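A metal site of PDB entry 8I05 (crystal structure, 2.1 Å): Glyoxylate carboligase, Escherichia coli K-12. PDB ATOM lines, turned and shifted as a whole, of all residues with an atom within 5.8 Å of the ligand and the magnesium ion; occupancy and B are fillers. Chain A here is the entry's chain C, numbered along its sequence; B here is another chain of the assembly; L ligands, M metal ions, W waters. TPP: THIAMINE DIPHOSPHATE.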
ATOM      1  N   ILE A 394      -9.207  12.779  31.339  1.00  0.00           N
ATOM      2  CA  ILE A 394      -8.477  12.615  30.072  1.00  0.00           C
ATOM      3  C   ILE A 394      -9.487  12.577  28.935  1.00  0.00           C
ATOM      4  O   ILE A 394     -10.671  12.336  29.133  1.00  0.00           O
ATOM      5  CB  ILE A 394      -7.589  11.336  30.094  1.00  0.00           C
ATOM      6  CG1 ILE A 394      -6.525  11.393  28.996  1.00  0.00           C
ATOM      7  CG2 ILE A 394      -8.422  10.088  29.913  1.00  0.00           C
ATOM      8  CD1 ILE A 394      -5.637  10.163  28.931  1.00  0.00           C
ATOM      9  N   GLY A 395      -9.004  12.785  27.719  1.00  0.00           N
ATOM     10  CA  GLY A 395      -9.838  12.899  26.551  1.00  0.00           C
ATOM     11  C   GLY A 395      -9.727  14.279  25.905  1.00  0.00           C
ATOM     12  O   GLY A 395      -9.130  15.207  26.454  1.00  0.00           O
ATOM     13  N   LEU A 396     -10.311  14.376  24.708  1.00  0.00           N
ATOM     14  CA  LEU A 396     -10.352  15.686  24.062  1.00  0.00           C
ATOM     15  C   LEU A 396     -11.075  16.688  24.943  1.00  0.00           C
ATOM     16  O   LEU A 396     -10.728  17.871  24.971  1.00  0.00           O
ATOM     17  CB  LEU A 396     -11.010  15.568  22.692  1.00  0.00           C
ATOM     18  CG  LEU A 396     -10.209  14.744  21.674  1.00  0.00           C
ATOM     19  CD1 LEU A 396     -10.851  14.759  20.323  1.00  0.00           C
ATOM     20  CD2 LEU A 396      -8.763  15.252  21.599  1.00  0.00           C
ATOM     21  N   SER A 397     -12.048  16.215  25.729  1.00  0.00           N
ATOM     22  CA  SER A 397     -12.745  17.072  26.691  1.00  0.00           C
ATOM     23  C   SER A 397     -11.774  17.722  27.656  1.00  0.00           C
ATOM     24  O   SER A 397     -11.844  18.930  27.906  1.00  0.00           O
ATOM     25  CB  SER A 397     -13.756  16.223  27.474  1.00  0.00           C
ATOM     26  OG  SER A 397     -13.106  15.054  27.984  1.00  0.00           O
ATOM     27  N   GLN A 398     -10.840  16.932  28.182  1.00  0.00           N
ATOM     28  CA  GLN A 398      -9.901  17.394  29.202  1.00  0.00           C
ATOM     29  C   GLN A 398      -8.753  18.182  28.586  1.00  0.00           C
ATOM     30  O   GLN A 398      -8.279  19.161  29.177  1.00  0.00           O
ATOM     31  CB  GLN A 398      -9.366  16.183  29.993  1.00  0.00           C
ATOM     32  CG  GLN A 398      -8.270  16.496  31.021  1.00  0.00           C
ATOM     33  CD  GLN A 398      -6.854  16.249  30.489  1.00  0.00           C
ATOM     34  OE1 GLN A 398      -6.680  15.689  29.406  1.00  0.00           O
ATOM     35  NE2 GLN A 398      -5.834  16.649  31.266  1.00  0.00           N
ATOM     36  N   ALA A 419      -1.541   9.328  35.165  1.00  0.00           N
ATOM     37  CA  ALA A 419      -2.155   8.027  34.894  1.00  0.00           C
ATOM     38  C   ALA A 419      -3.443   8.112  34.080  1.00  0.00           C
ATOM     39  O   ALA A 419      -3.724   7.209  33.293  1.00  0.00           O
ATOM     40  CB  ALA A 419      -2.457   7.279  36.195  1.00  0.00           C
ATOM     41  N   GLY A 420      -4.247   9.158  34.267  1.00  0.00           N
ATOM     42  CA  GLY A 420      -5.479   9.355  33.531  1.00  0.00           C
ATOM     43  C   GLY A 420      -6.422   8.152  33.396  1.00  0.00           C
ATOM     44  O   GLY A 420      -6.780   7.767  32.284  1.00  0.00           O
ATOM     45  N   PRO A 421      -6.828   7.537  34.507  1.00  0.00           N
ATOM     46  CA  PRO A 421      -7.799   6.436  34.424  1.00  0.00           C
ATOM     47  C   PRO A 421      -9.205   6.936  34.130  1.00  0.00           C
ATOM     48  O   PRO A 421      -9.752   7.745  34.870  1.00  0.00           O
ATOM     49  CB  PRO A 421      -7.757   5.806  35.815  1.00  0.00           C
ATOM     50  CG  PRO A 421      -7.334   6.946  36.716  1.00  0.00           C
ATOM     51  CD  PRO A 421      -6.369   7.768  35.886  1.00  0.00           C
ATOM     52  N   LEU A 422      -9.814   6.384  33.081  1.00  0.00           N
ATOM     53  CA  LEU A 422     -11.191   6.724  32.757  1.00  0.00           C
ATOM     54  C   LEU A 422     -12.084   6.340  33.939  1.00  0.00           C
ATOM     55  O   LEU A 422     -11.840   5.330  34.618  1.00  0.00           O
ATOM     56  CB  LEU A 422     -11.641   6.018  31.477  1.00  0.00           C
ATOM     57  CG  LEU A 422     -11.047   6.599  30.176  1.00  0.00           C
ATOM     58  CD1 LEU A 422     -11.370   5.755  28.981  1.00  0.00           C
ATOM     59  CD2 LEU A 422     -11.546   8.024  29.970  1.00  0.00           C
ATOM     60  N   SER A 445     -16.248  15.973  31.837  1.00  0.00           N
ATOM     61  CA  SER A 445     -16.044  14.637  31.278  1.00  0.00           C
ATOM     62  C   SER A 445     -16.444  14.601  29.810  1.00  0.00           C
ATOM     63  O   SER A 445     -17.342  15.341  29.376  1.00  0.00           O
ATOM     64  CB  SER A 445     -16.887  13.582  32.003  1.00  0.00           C
ATOM     65  OG  SER A 445     -16.336  13.240  33.265  1.00  0.00           O
ATOM     66  N   GLY A 446     -15.785  13.711  29.052  1.00  0.00           N
ATOM     67  CA  GLY A 446     -16.369  13.213  27.822  1.00  0.00           C
ATOM     68  C   GLY A 446     -17.407  12.137  28.128  1.00  0.00           C
ATOM     69  O   GLY A 446     -17.544  11.722  29.284  1.00  0.00           O
ATOM     70  N   ASP A 447     -18.136  11.688  27.095  1.00  0.00           N
ATOM     71  CA  ASP A 447     -19.172  10.687  27.350  1.00  0.00           C
ATOM     72  C   ASP A 447     -18.581   9.355  27.808  1.00  0.00           C
ATOM     73  O   ASP A 447     -19.141   8.708  28.696  1.00  0.00           O
ATOM     74  CB  ASP A 447     -20.089  10.493  26.124  1.00  0.00           C
ATOM     75  CG  ASP A 447     -19.330  10.425  24.798  1.00  0.00           C
ATOM     76  OD1 ASP A 447     -18.404  11.245  24.574  1.00  0.00           O
ATOM     77  OD2 ASP A 447     -19.678   9.550  23.983  1.00  0.00           O
ATOM     78  N   PHE A 448     -17.439   8.941  27.269  1.00  0.00           N
ATOM     79  CA  PHE A 448     -16.882   7.631  27.613  1.00  0.00           C
ATOM     80  C   PHE A 448     -16.384   7.628  29.063  1.00  0.00           C
ATOM     81  O   PHE A 448     -16.754   6.753  29.859  1.00  0.00           O
ATOM     82  CB  PHE A 448     -15.749   7.268  26.648  1.00  0.00           C
ATOM     83  CG  PHE A 448     -15.429   5.791  26.573  1.00  0.00           C
ATOM     84  CD1 PHE A 448     -16.412   4.845  26.342  1.00  0.00           C
ATOM     85  CD2 PHE A 448     -14.111   5.376  26.662  1.00  0.00           C
ATOM     86  CE1 PHE A 448     -16.091   3.495  26.243  1.00  0.00           C
ATOM     87  CE2 PHE A 448     -13.785   4.042  26.566  1.00  0.00           C
ATOM     88  CZ  PHE A 448     -14.781   3.093  26.352  1.00  0.00           C
ATOM     89  N   ASP A 449     -15.600   8.631  29.440  1.00  0.00           N
ATOM     90  CA  ASP A 449     -15.159   8.757  30.822  1.00  0.00           C
ATOM     91  C   ASP A 449     -16.365   8.779  31.765  1.00  0.00           C
ATOM     92  O   ASP A 449     -16.351   8.126  32.814  1.00  0.00           O
ATOM     93  CB  ASP A 449     -14.295  10.018  30.961  1.00  0.00           C
ATOM     94  CG  ASP A 449     -14.127  10.513  32.391  1.00  0.00           C
ATOM     95  OD1 ASP A 449     -13.738   9.735  33.295  1.00  0.00           O
ATOM     96  OD2 ASP A 449     -14.335  11.726  32.609  1.00  0.00           O
ATOM     97  N   PHE A 450     -17.436   9.443  31.342  1.00  0.00           N
ATOM     98  CA  PHE A 450     -18.621   9.580  32.194  1.00  0.00           C
ATOM     99  C   PHE A 450     -19.286   8.236  32.448  1.00  0.00           C
ATOM    100  O   PHE A 450     -19.867   8.028  33.525  1.00  0.00           O
ATOM    101  CB  PHE A 450     -19.613  10.540  31.535  1.00  0.00           C
ATOM    102  CG  PHE A 450     -20.733  11.008  32.424  1.00  0.00           C
ATOM    103  CD1 PHE A 450     -20.490  11.894  33.469  1.00  0.00           C
ATOM    104  CD2 PHE A 450     -22.039  10.623  32.186  1.00  0.00           C
ATOM    105  CE1 PHE A 450     -21.526  12.334  34.256  1.00  0.00           C
ATOM    106  CE2 PHE A 450     -23.076  11.063  32.973  1.00  0.00           C
ATOM    107  CZ  PHE A 450     -22.835  11.916  34.004  1.00  0.00           C
ATOM    108  N   PHE A 452     -17.872   5.078  32.632  1.00  0.00           N
ATOM    109  CA  PHE A 452     -17.098   4.033  33.311  1.00  0.00           C
ATOM    110  C   PHE A 452     -17.626   3.765  34.719  1.00  0.00           C
ATOM    111  O   PHE A 452     -17.858   2.613  35.104  1.00  0.00           O
ATOM    112  CB  PHE A 452     -15.630   4.446  33.410  1.00  0.00           C
ATOM    113  CG  PHE A 452     -14.737   3.840  32.368  1.00  0.00           C
ATOM    114  CD1 PHE A 452     -15.015   3.973  31.019  1.00  0.00           C
ATOM    115  CD2 PHE A 452     -13.590   3.162  32.738  1.00  0.00           C
ATOM    116  CE1 PHE A 452     -14.164   3.431  30.061  1.00  0.00           C
ATOM    117  CE2 PHE A 452     -12.737   2.607  31.784  1.00  0.00           C
ATOM    118  CZ  PHE A 452     -13.035   2.757  30.452  1.00  0.00           C
ATOM    119  N   VAL A 472     -19.598  16.625  27.899  1.00  0.00           N
ATOM    120  CA  VAL A 472     -19.508  16.981  26.486  1.00  0.00           C
ATOM    121  C   VAL A 472     -19.553  15.680  25.692  1.00  0.00           C
ATOM    122  O   VAL A 472     -18.614  14.876  25.720  1.00  0.00           O
ATOM    123  CB  VAL A 472     -18.245  17.815  26.181  1.00  0.00           C
ATOM    124  CG1 VAL A 472     -18.380  19.219  26.790  1.00  0.00           C
ATOM    125  CG2 VAL A 472     -16.988  17.177  26.742  1.00  0.00           C
ATOM    126  N   ASN A 473     -20.672  15.458  25.004  1.00  0.00           N
ATOM    127  CA  ASN A 473     -20.993  14.167  24.400  1.00  0.00           C
ATOM    128  C   ASN A 473     -20.789  14.241  22.894  1.00  0.00           C
ATOM    129  O   ASN A 473     -21.499  14.987  22.205  1.00  0.00           O
ATOM    130  CB  ASN A 473     -22.441  13.772  24.733  1.00  0.00           C
ATOM    131  CG  ASN A 473     -22.850  12.432  24.125  1.00  0.00           C
ATOM    132  OD1 ASN A 473     -22.040  11.712  23.533  1.00  0.00           O
ATOM    133  ND2 ASN A 473     -24.124  12.084  24.298  1.00  0.00           N
ATOM    134  N   ASN A 474     -19.808  13.492  22.387  1.00  0.00           N
ATOM    135  CA  ASN A 474     -19.637  13.346  20.951  1.00  0.00           C
ATOM    136  C   ASN A 474     -19.915  11.927  20.449  1.00  0.00           C
ATOM    137  O   ASN A 474     -19.593  11.621  19.290  1.00  0.00           O
ATOM    138  CB  ASN A 474     -18.211  13.764  20.554  1.00  0.00           C
ATOM    139  CG  ASN A 474     -17.154  13.040  21.355  1.00  0.00           C
ATOM    140  OD1 ASN A 474     -17.426  12.001  21.962  1.00  0.00           O
ATOM    141  ND2 ASN A 474     -15.940  13.597  21.387  1.00  0.00           N
ATOM    142  N   ALA A 475     -20.485  11.062  21.283  1.00  0.00           N
ATOM    143  CA  ALA A 475     -20.704   9.640  20.953  1.00  0.00           C
ATOM    144  C   ALA A 475     -19.452   8.992  20.355  1.00  0.00           C
ATOM    145  O   ALA A 475     -19.526   8.176  19.433  1.00  0.00           O
ATOM    146  CB  ALA A 475     -21.899   9.468  20.011  1.00  0.00           C
ATOM    147  N   TYR A 476     -18.292   9.367  20.897  1.00  0.00           N
ATOM    148  CA  TYR A 476     -16.989   8.943  20.383  1.00  0.00           C
ATOM    149  C   TYR A 476     -15.998   8.781  21.530  1.00  0.00           C
ATOM    150  O   TYR A 476     -16.074   9.498  22.528  1.00  0.00           O
ATOM    151  CB  TYR A 476     -16.404   9.987  19.422  1.00  0.00           C
ATOM    152  CG  TYR A 476     -16.352   9.654  17.951  1.00  0.00           C
ATOM    153  CD1 TYR A 476     -15.443   8.730  17.459  1.00  0.00           C
ATOM    154  CD2 TYR A 476     -17.142  10.340  17.044  1.00  0.00           C
ATOM    155  CE1 TYR A 476     -15.368   8.460  16.094  1.00  0.00           C
ATOM    156  CE2 TYR A 476     -17.076  10.097  15.695  1.00  0.00           C
ATOM    157  CZ  TYR A 476     -16.190   9.147  15.225  1.00  0.00           C
ATOM    158  OH  TYR A 476     -16.136   8.895  13.877  1.00  0.00           O
ATOM    159  N   LEU A 477     -15.021   7.882  21.348  1.00  0.00           N
ATOM    160  CA  LEU A 477     -13.754   8.004  22.066  1.00  0.00           C
ATOM    161  C   LEU A 477     -12.895   8.971  21.265  1.00  0.00           C
ATOM    162  O   LEU A 477     -12.027   8.579  20.480  1.00  0.00           O
ATOM    163  CB  LEU A 477     -13.049   6.665  22.232  1.00  0.00           C
ATOM    164  CG  LEU A 477     -13.715   5.303  22.401  1.00  0.00           C
ATOM    165  CD1 LEU A 477     -12.701   4.266  22.939  1.00  0.00           C
ATOM    166  CD2 LEU A 477     -14.994   5.361  23.221  1.00  0.00           C
ATOM    167  N   GLY A 478     -13.150  10.266  21.454  1.00  0.00           N
ATOM    168  CA  GLY A 478     -12.662  11.251  20.504  1.00  0.00           C
ATOM    169  C   GLY A 478     -11.149  11.329  20.456  1.00  0.00           C
ATOM    170  O   GLY A 478     -10.559  11.418  19.372  1.00  0.00           O
ATOM    171  N   LEU A 479     -10.494  11.287  21.611  1.00  0.00           N
ATOM    172  CA  LEU A 479      -9.037  11.339  21.623  1.00  0.00           C
ATOM    173  C   LEU A 479      -8.448  10.152  20.867  1.00  0.00           C
ATOM    174  O   LEU A 479      -7.420  10.304  20.203  1.00  0.00           O
ATOM    175  CB  LEU A 479      -8.504  11.395  23.055  1.00  0.00           C
ATOM    176  CG  LEU A 479      -6.973  11.436  23.225  1.00  0.00           C
ATOM    177  CD1 LEU A 479      -6.313  12.573  22.424  1.00  0.00           C
ATOM    178  CD2 LEU A 479      -6.581  11.530  24.695  1.00  0.00           C
ATOM    179  N   ILE A 480      -9.109   8.995  20.925  1.00  0.00           N
ATOM    180  CA  ILE A 480      -8.535   7.825  20.259  1.00  0.00           C
ATOM    181  C   ILE A 480      -8.819   7.869  18.764  1.00  0.00           C
ATOM    182  O   ILE A 480      -7.978   7.439  17.962  1.00  0.00           O
ATOM    183  CB  ILE A 480      -9.036   6.503  20.873  1.00  0.00           C
ATOM    184  CG1 ILE A 480      -8.871   6.528  22.399  1.00  0.00           C
ATOM    185  CG2 ILE A 480      -8.268   5.320  20.290  1.00  0.00           C
ATOM    186  CD1 ILE A 480      -7.488   7.037  22.877  1.00  0.00           C
ATOM    187  N   LEU A 495     -19.492   5.194  19.846  1.00  0.00           N
ATOM    188  CA  LEU A 495     -20.452   4.776  20.866  1.00  0.00           C
ATOM    189  C   LEU A 495     -21.894   4.991  20.448  1.00  0.00           C
ATOM    190  O   LEU A 495     -22.804   4.670  21.223  1.00  0.00           O
ATOM    191  CB  LEU A 495     -20.191   5.547  22.164  1.00  0.00           C
ATOM    192  CG  LEU A 495     -18.772   5.362  22.691  1.00  0.00           C
ATOM    193  CD1 LEU A 495     -18.470   6.364  23.779  1.00  0.00           C
ATOM    194  CD2 LEU A 495     -18.619   3.924  23.212  1.00  0.00           C
ATOM    195  N   LEU A 556     -22.191  17.603  21.313  1.00  0.00           N
ATOM    196  CA  LEU A 556     -21.161  18.143  20.431  1.00  0.00           C
ATOM    197  C   LEU A 556     -21.335  17.610  19.023  1.00  0.00           C
ATOM    198  O   LEU A 556     -22.016  16.605  18.800  1.00  0.00           O
ATOM    199  CB  LEU A 556     -19.763  17.772  20.936  1.00  0.00           C
ATOM    200  CG  LEU A 556     -19.351  18.139  22.343  1.00  0.00           C
ATOM    201  CD1 LEU A 556     -17.913  17.685  22.580  1.00  0.00           C
ATOM    202  CD2 LEU A 556     -19.512  19.656  22.567  1.00  0.00           C
ATOM    203  N   VAL B  26     -10.939  -2.032  24.788  1.00  0.00           N
ATOM    204  CA  VAL B  26     -11.026  -0.572  24.741  1.00  0.00           C
ATOM    205  C   VAL B  26      -9.746  -0.080  24.099  1.00  0.00           C
ATOM    206  O   VAL B  26      -8.664  -0.258  24.683  1.00  0.00           O
ATOM    207  CB  VAL B  26     -11.195   0.016  26.144  1.00  0.00           C
ATOM    208  CG1 VAL B  26     -11.185   1.547  26.096  1.00  0.00           C
ATOM    209  CG2 VAL B  26     -12.458  -0.497  26.806  1.00  0.00           C
ATOM    210  N   PRO B  27      -9.786   0.520  22.910  1.00  0.00           N
ATOM    211  CA  PRO B  27      -8.556   1.009  22.280  1.00  0.00           C
ATOM    212  C   PRO B  27      -7.983   2.234  22.984  1.00  0.00           C
ATOM    213  O   PRO B  27      -8.652   2.936  23.739  1.00  0.00           O
ATOM    214  CB  PRO B  27      -9.011   1.358  20.853  1.00  0.00           C
ATOM    215  CG  PRO B  27     -10.447   1.711  21.026  1.00  0.00           C
ATOM    216  CD  PRO B  27     -10.974   0.789  22.075  1.00  0.00           C
ATOM    217  N   GLY B  28      -6.701   2.459  22.744  1.00  0.00           N
ATOM    218  CA  GLY B  28      -6.027   3.673  23.173  1.00  0.00           C
ATOM    219  C   GLY B  28      -4.807   3.866  22.299  1.00  0.00           C
ATOM    220  O   GLY B  28      -4.462   3.010  21.479  1.00  0.00           O
ATOM    221  N   ALA B  29      -4.131   5.006  22.502  1.00  0.00           N
ATOM    222  CA  ALA B  29      -3.039   5.354  21.598  1.00  0.00           C
ATOM    223  C   ALA B  29      -1.963   4.283  21.598  1.00  0.00           C
ATOM    224  O   ALA B  29      -1.428   3.929  20.546  1.00  0.00           O
ATOM    225  CB  ALA B  29      -2.448   6.722  21.980  1.00  0.00           C
ATOM    226  N   VAL B  52     -12.848  -0.846  31.066  1.00  0.00           N
ATOM    227  CA  VAL B  52     -11.862  -1.887  30.774  1.00  0.00           C
ATOM    228  C   VAL B  52     -12.120  -3.104  31.651  1.00  0.00           C
ATOM    229  O   VAL B  52     -11.979  -4.241  31.191  1.00  0.00           O
ATOM    230  CB  VAL B  52     -10.414  -1.369  30.932  1.00  0.00           C
ATOM    231  CG1 VAL B  52      -9.419  -2.540  30.974  1.00  0.00           C
ATOM    232  CG2 VAL B  52     -10.057  -0.456  29.767  1.00  0.00           C
ATOM    233  N   THR B  76      -5.184  -0.372  26.427  1.00  0.00           N
ATOM    234  CA  THR B  76      -3.998   0.453  26.168  1.00  0.00           C
ATOM    235  C   THR B  76      -3.033   0.340  27.342  1.00  0.00           C
ATOM    236  O   THR B  76      -3.131  -0.590  28.146  1.00  0.00           O
ATOM    237  CB  THR B  76      -4.406   1.915  25.904  1.00  0.00           C
ATOM    238  OG1 THR B  76      -3.275   2.645  25.399  1.00  0.00           O
ATOM    239  CG2 THR B  76      -4.930   2.620  27.160  1.00  0.00           C
ATOM    240  N   PRO B  79      -3.322   2.712  32.984  1.00  0.00           N
ATOM    241  CA  PRO B  79      -4.489   2.312  33.790  1.00  0.00           C
ATOM    242  C   PRO B  79      -5.313   1.173  33.199  1.00  0.00           C
ATOM    243  O   PRO B  79      -6.054   0.517  33.951  1.00  0.00           O
ATOM    244  CB  PRO B  79      -5.298   3.617  33.904  1.00  0.00           C
ATOM    245  CG  PRO B  79      -4.942   4.372  32.681  1.00  0.00           C
ATOM    246  CD  PRO B  79      -3.475   4.063  32.421  1.00  0.00           C
ATOM    247  N   ALA B  80      -5.312   0.985  31.886  1.00  0.00           N
ATOM    248  CA  ALA B  80      -6.086  -0.121  31.334  1.00  0.00           C
ATOM    249  C   ALA B  80      -5.588  -1.462  31.872  1.00  0.00           C
ATOM    250  O   ALA B  80      -6.380  -2.315  32.257  1.00  0.00           O
ATOM    251  CB  ALA B  80      -6.040  -0.109  29.801  1.00  0.00           C
ATOM    252  N   ASP B  83      -6.687  -1.943  35.436  1.00  0.00           N
ATOM    253  CA  ASP B  83      -8.111  -2.270  35.488  1.00  0.00           C
ATOM    254  C   ASP B  83      -8.394  -3.737  35.156  1.00  0.00           C
ATOM    255  O   ASP B  83      -9.540  -4.174  35.328  1.00  0.00           O
ATOM    256  CB  ASP B  83      -8.926  -1.416  34.506  1.00  0.00           C
ATOM    257  CG  ASP B  83      -9.252  -0.013  35.037  1.00  0.00           C
ATOM    258  OD1 ASP B  83      -9.097   0.276  36.251  1.00  0.00           O
ATOM    259  OD2 ASP B  83      -9.682   0.815  34.192  1.00  0.00           O
ATOM    260  N   GLN B 116       1.429   7.612  31.121  1.00  0.00           N
ATOM    261  CA  GLN B 116       0.575   6.427  31.258  1.00  0.00           C
ATOM    262  C   GLN B 116       1.354   5.126  31.048  1.00  0.00           C
ATOM    263  O   GLN B 116       0.882   4.198  30.401  1.00  0.00           O
ATOM    264  CB  GLN B 116      -0.617   6.486  30.294  1.00  0.00           C
ATOM    265  CG  GLN B 116      -1.746   7.391  30.732  1.00  0.00           C
ATOM    266  CD  GLN B 116      -3.028   7.186  29.939  1.00  0.00           C
ATOM    267  OE1 GLN B 116      -2.995   7.012  28.711  1.00  0.00           O
ATOM    268  NE2 GLN B 116      -4.165   7.206  30.625  1.00  0.00           N
HETATM  269  N1' TPP L   1      -8.646   2.831  29.143  1.00  0.00           N
HETATM  270  C2' TPP L   1      -8.549   3.444  30.349  1.00  0.00           C
HETATM  271  CM2 TPP L   1      -8.986   2.666  31.550  1.00  0.00           C
HETATM  272  N3' TPP L   1      -8.088   4.672  30.560  1.00  0.00           N
HETATM  273  C4' TPP L   1      -7.688   5.396  29.490  1.00  0.00           C
HETATM  274  N4' TPP L   1      -7.234   6.623  29.724  1.00  0.00           N
HETATM  275  C5' TPP L   1      -7.767   4.841  28.173  1.00  0.00           C
HETATM  276  C6' TPP L   1      -8.265   3.558  28.093  1.00  0.00           C
HETATM  277  C7' TPP L   1      -7.326   5.586  26.933  1.00  0.00           C
HETATM  278  N3  TPP L   1      -8.170   6.773  26.610  1.00  0.00           N
HETATM  279  C2  TPP L   1      -7.787   8.022  26.823  1.00  0.00           C
HETATM  280  S1  TPP L   1      -8.953   9.138  26.333  1.00  0.00           S
HETATM  281  C5  TPP L   1     -10.001   7.880  25.800  1.00  0.00           C
HETATM  282  C4  TPP L   1      -9.436   6.652  26.019  1.00  0.00           C
HETATM  283  CM4 TPP L   1     -10.011   5.306  25.706  1.00  0.00           C
HETATM  284  C6  TPP L   1     -11.361   8.205  25.223  1.00  0.00           C
HETATM  285  C7  TPP L   1     -11.969   9.428  25.858  1.00  0.00           C
HETATM  286  O7  TPP L   1     -13.350   9.549  25.426  1.00  0.00           O
HETATM  287  PA  TPP L   1     -14.372  10.568  26.058  1.00  0.00           P
HETATM  288  O1A TPP L   1     -14.237  10.504  27.592  1.00  0.00           O
HETATM  289  O2A TPP L   1     -15.729  10.428  25.485  1.00  0.00           O
HETATM  290  O3A TPP L   1     -13.723  11.884  25.561  1.00  0.00           O
HETATM  291  PB  TPP L   1     -13.487  12.640  24.189  1.00  0.00           P
HETATM  292  O1B TPP L   1     -14.333  12.014  23.130  1.00  0.00           O
HETATM  293  O2B TPP L   1     -13.866  14.148  24.495  1.00  0.00           O
HETATM  294  O3B TPP L   1     -11.965  12.505  23.918  1.00  0.00           O
HETATM  295 MG    MG M   1     -16.302  11.298  23.685  1.00  0.00          MG
HETATM  296  O   HOH W   1      -7.772   0.506  27.166  1.00  0.00           O
HETATM  297  O   HOH W   2     -13.428  12.544  28.805  1.00  0.00           O
HETATM  298  O   HOH W   3     -16.467  13.497  24.387  1.00  0.00           O
HETATM  299  O   HOH W   4     -14.779  16.426  23.095  1.00  0.00           O
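Ile 394 touches the ligand (CG2 to N4', 3.7 Å).
Gly 395 touches the ligand (CA to O3B, 3.4 Å).
Leu 422 touches the ligand.
Gly 446 touches the ligand (CA to O1A, 3.5 Å).
Phe 452 touches the ligand.
Leu 477 touches the ligand (CA to O7, 3.7 Å).
CG1 of Ile 480 touches C4 of the ligand, 3.7 Å away.
CG1 of Val 26 of chain B touches CM4 of the ligand (3.96 Å).
Pro 27 of chain B touches the ligand (O to CM4, 3.4 Å).
Val 52 of chain B touches the ligand.
Thr 76 of chain B touches the ligand (CG2 to C6', 3.6 Å).
Pro 79 of chain B touches the ligand (CG to N3', 3.8 Å).
Ala 80 of chain B touches the ligand (CB to N1', 3.98 Å).
OD2 of Asp 83 of chain B touches CM2 of the ligand, 3.3 Å away.
Hydrophobic or aromatic side chains within 4 Å of the ligand: Ile 394, Leu 396, Leu 422, Phe 448, Phe 452, Leu 477, Leu 479, Ile 480, Val 26 of chain B, Val 52 of chain B, Pro 79 of chain B and Ala 80 of chain B.
Of the 37 residues printed, 25 come within 4 Å of the ligand.
The magnesium ion is bound by O2A of the ligand (2.1 Å), O of Tyr 476 (2.2 Å), O1B of the ligand (2.2 Å), OD1 of Asn 474 (2.2 Å), OD1 of Asp 447 (2.3 Å) and water W3 (2.3 Å).
Residues that only touch the magnesium ion: Gly 478.
Of the 37 residues printed, 4 come within 4 Å of the magnesium ion.
Along chain A the residues within 4 Å of the magnesium ion span positions 447 to 478.
The nearest printed residue that does not touch the magnesium ion is Leu 477 (4.3 Å).
An oxygen (O2A) of the ligand sits close to the backbone NH (N) of Asp 447, 3.2 Å away.
The backbone NH (N) of Leu 396 is in hydrogen-bond range of an oxygen (O3B) of the ligand, at 2.6 Å.
The backbone NH (N) of Gly 478 lies close to an oxygen (O1B) of the ligand, 2.7 Å away.
A nitrogen (N4') of the ligand sits at hydrogen-bond distance from the backbone carbonyl oxygen (O) of Gly 420, 2.8 Å away.
N of Phe 448 sits close to O2A of the ligand.
N of Asp 449 lies within hydrogen-bond range of O1A of the ligand.
An oxygen (O3B) of the ligand sits at hydrogen-bond distance from the backbone NH of Leu 479, at 3.0 Å.
The backbone NH (N) of Ser 397 sits at hydrogen-bond distance from an oxygen (O2B) of the ligand, 3.0 Å away.
N4' of the ligand lies close to NE2 of Gln 116 of chain B, at 3.3 Å.
The backbone NH (N) of Ala 475 sits at hydrogen-bond distance from the side-chain carboxylate (OD2) of Asp 447, at 3.2 Å.
OD1 of Asn 473 sits close to OD2 of Asp 447 (3.2 Å).
The side-chain amide nitrogen of Gln 116 of chain B sits at hydrogen-bond distance from the backbone carbonyl oxygen of Gly 420 (3.1 Å).
OD2 of Asp 449 lies within hydrogen-bond range of OG of Ser 445 (2.6 Å).
The side-chain hydroxyl of Ser 397 sits at hydrogen-bond distance from the backbone NH of Gly 446 (3.2 Å).
O of Ala 419 sits at hydrogen-bond distance from NE2 of Gln 116 of chain B, at 2.7 Å.
Water W3 lies within hydrogen-bond range of an oxygen (O2B) of the ligand (2.7 Å), the backbone carbonyl oxygen (O) of Val 472 (2.9 Å) and the side-chain amide nitrogen (ND2) of Asn 474 (3.0 Å).
Water W2 lies within hydrogen-bond range of O1A of the ligand (2.5 Å), N of Gly 446 (2.6 Å), OG of Ser 397 (2.7 Å) and O of Ile 394 (2.8 Å).
Water W1 lies within hydrogen-bond range of the backbone carbonyl oxygen (O) of Val 26 of chain B (2.7 Å), the backbone NH (N) of Thr 76 of chain B (2.8 Å) and a nitrogen (N1') of the ligand (3.2 Å).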
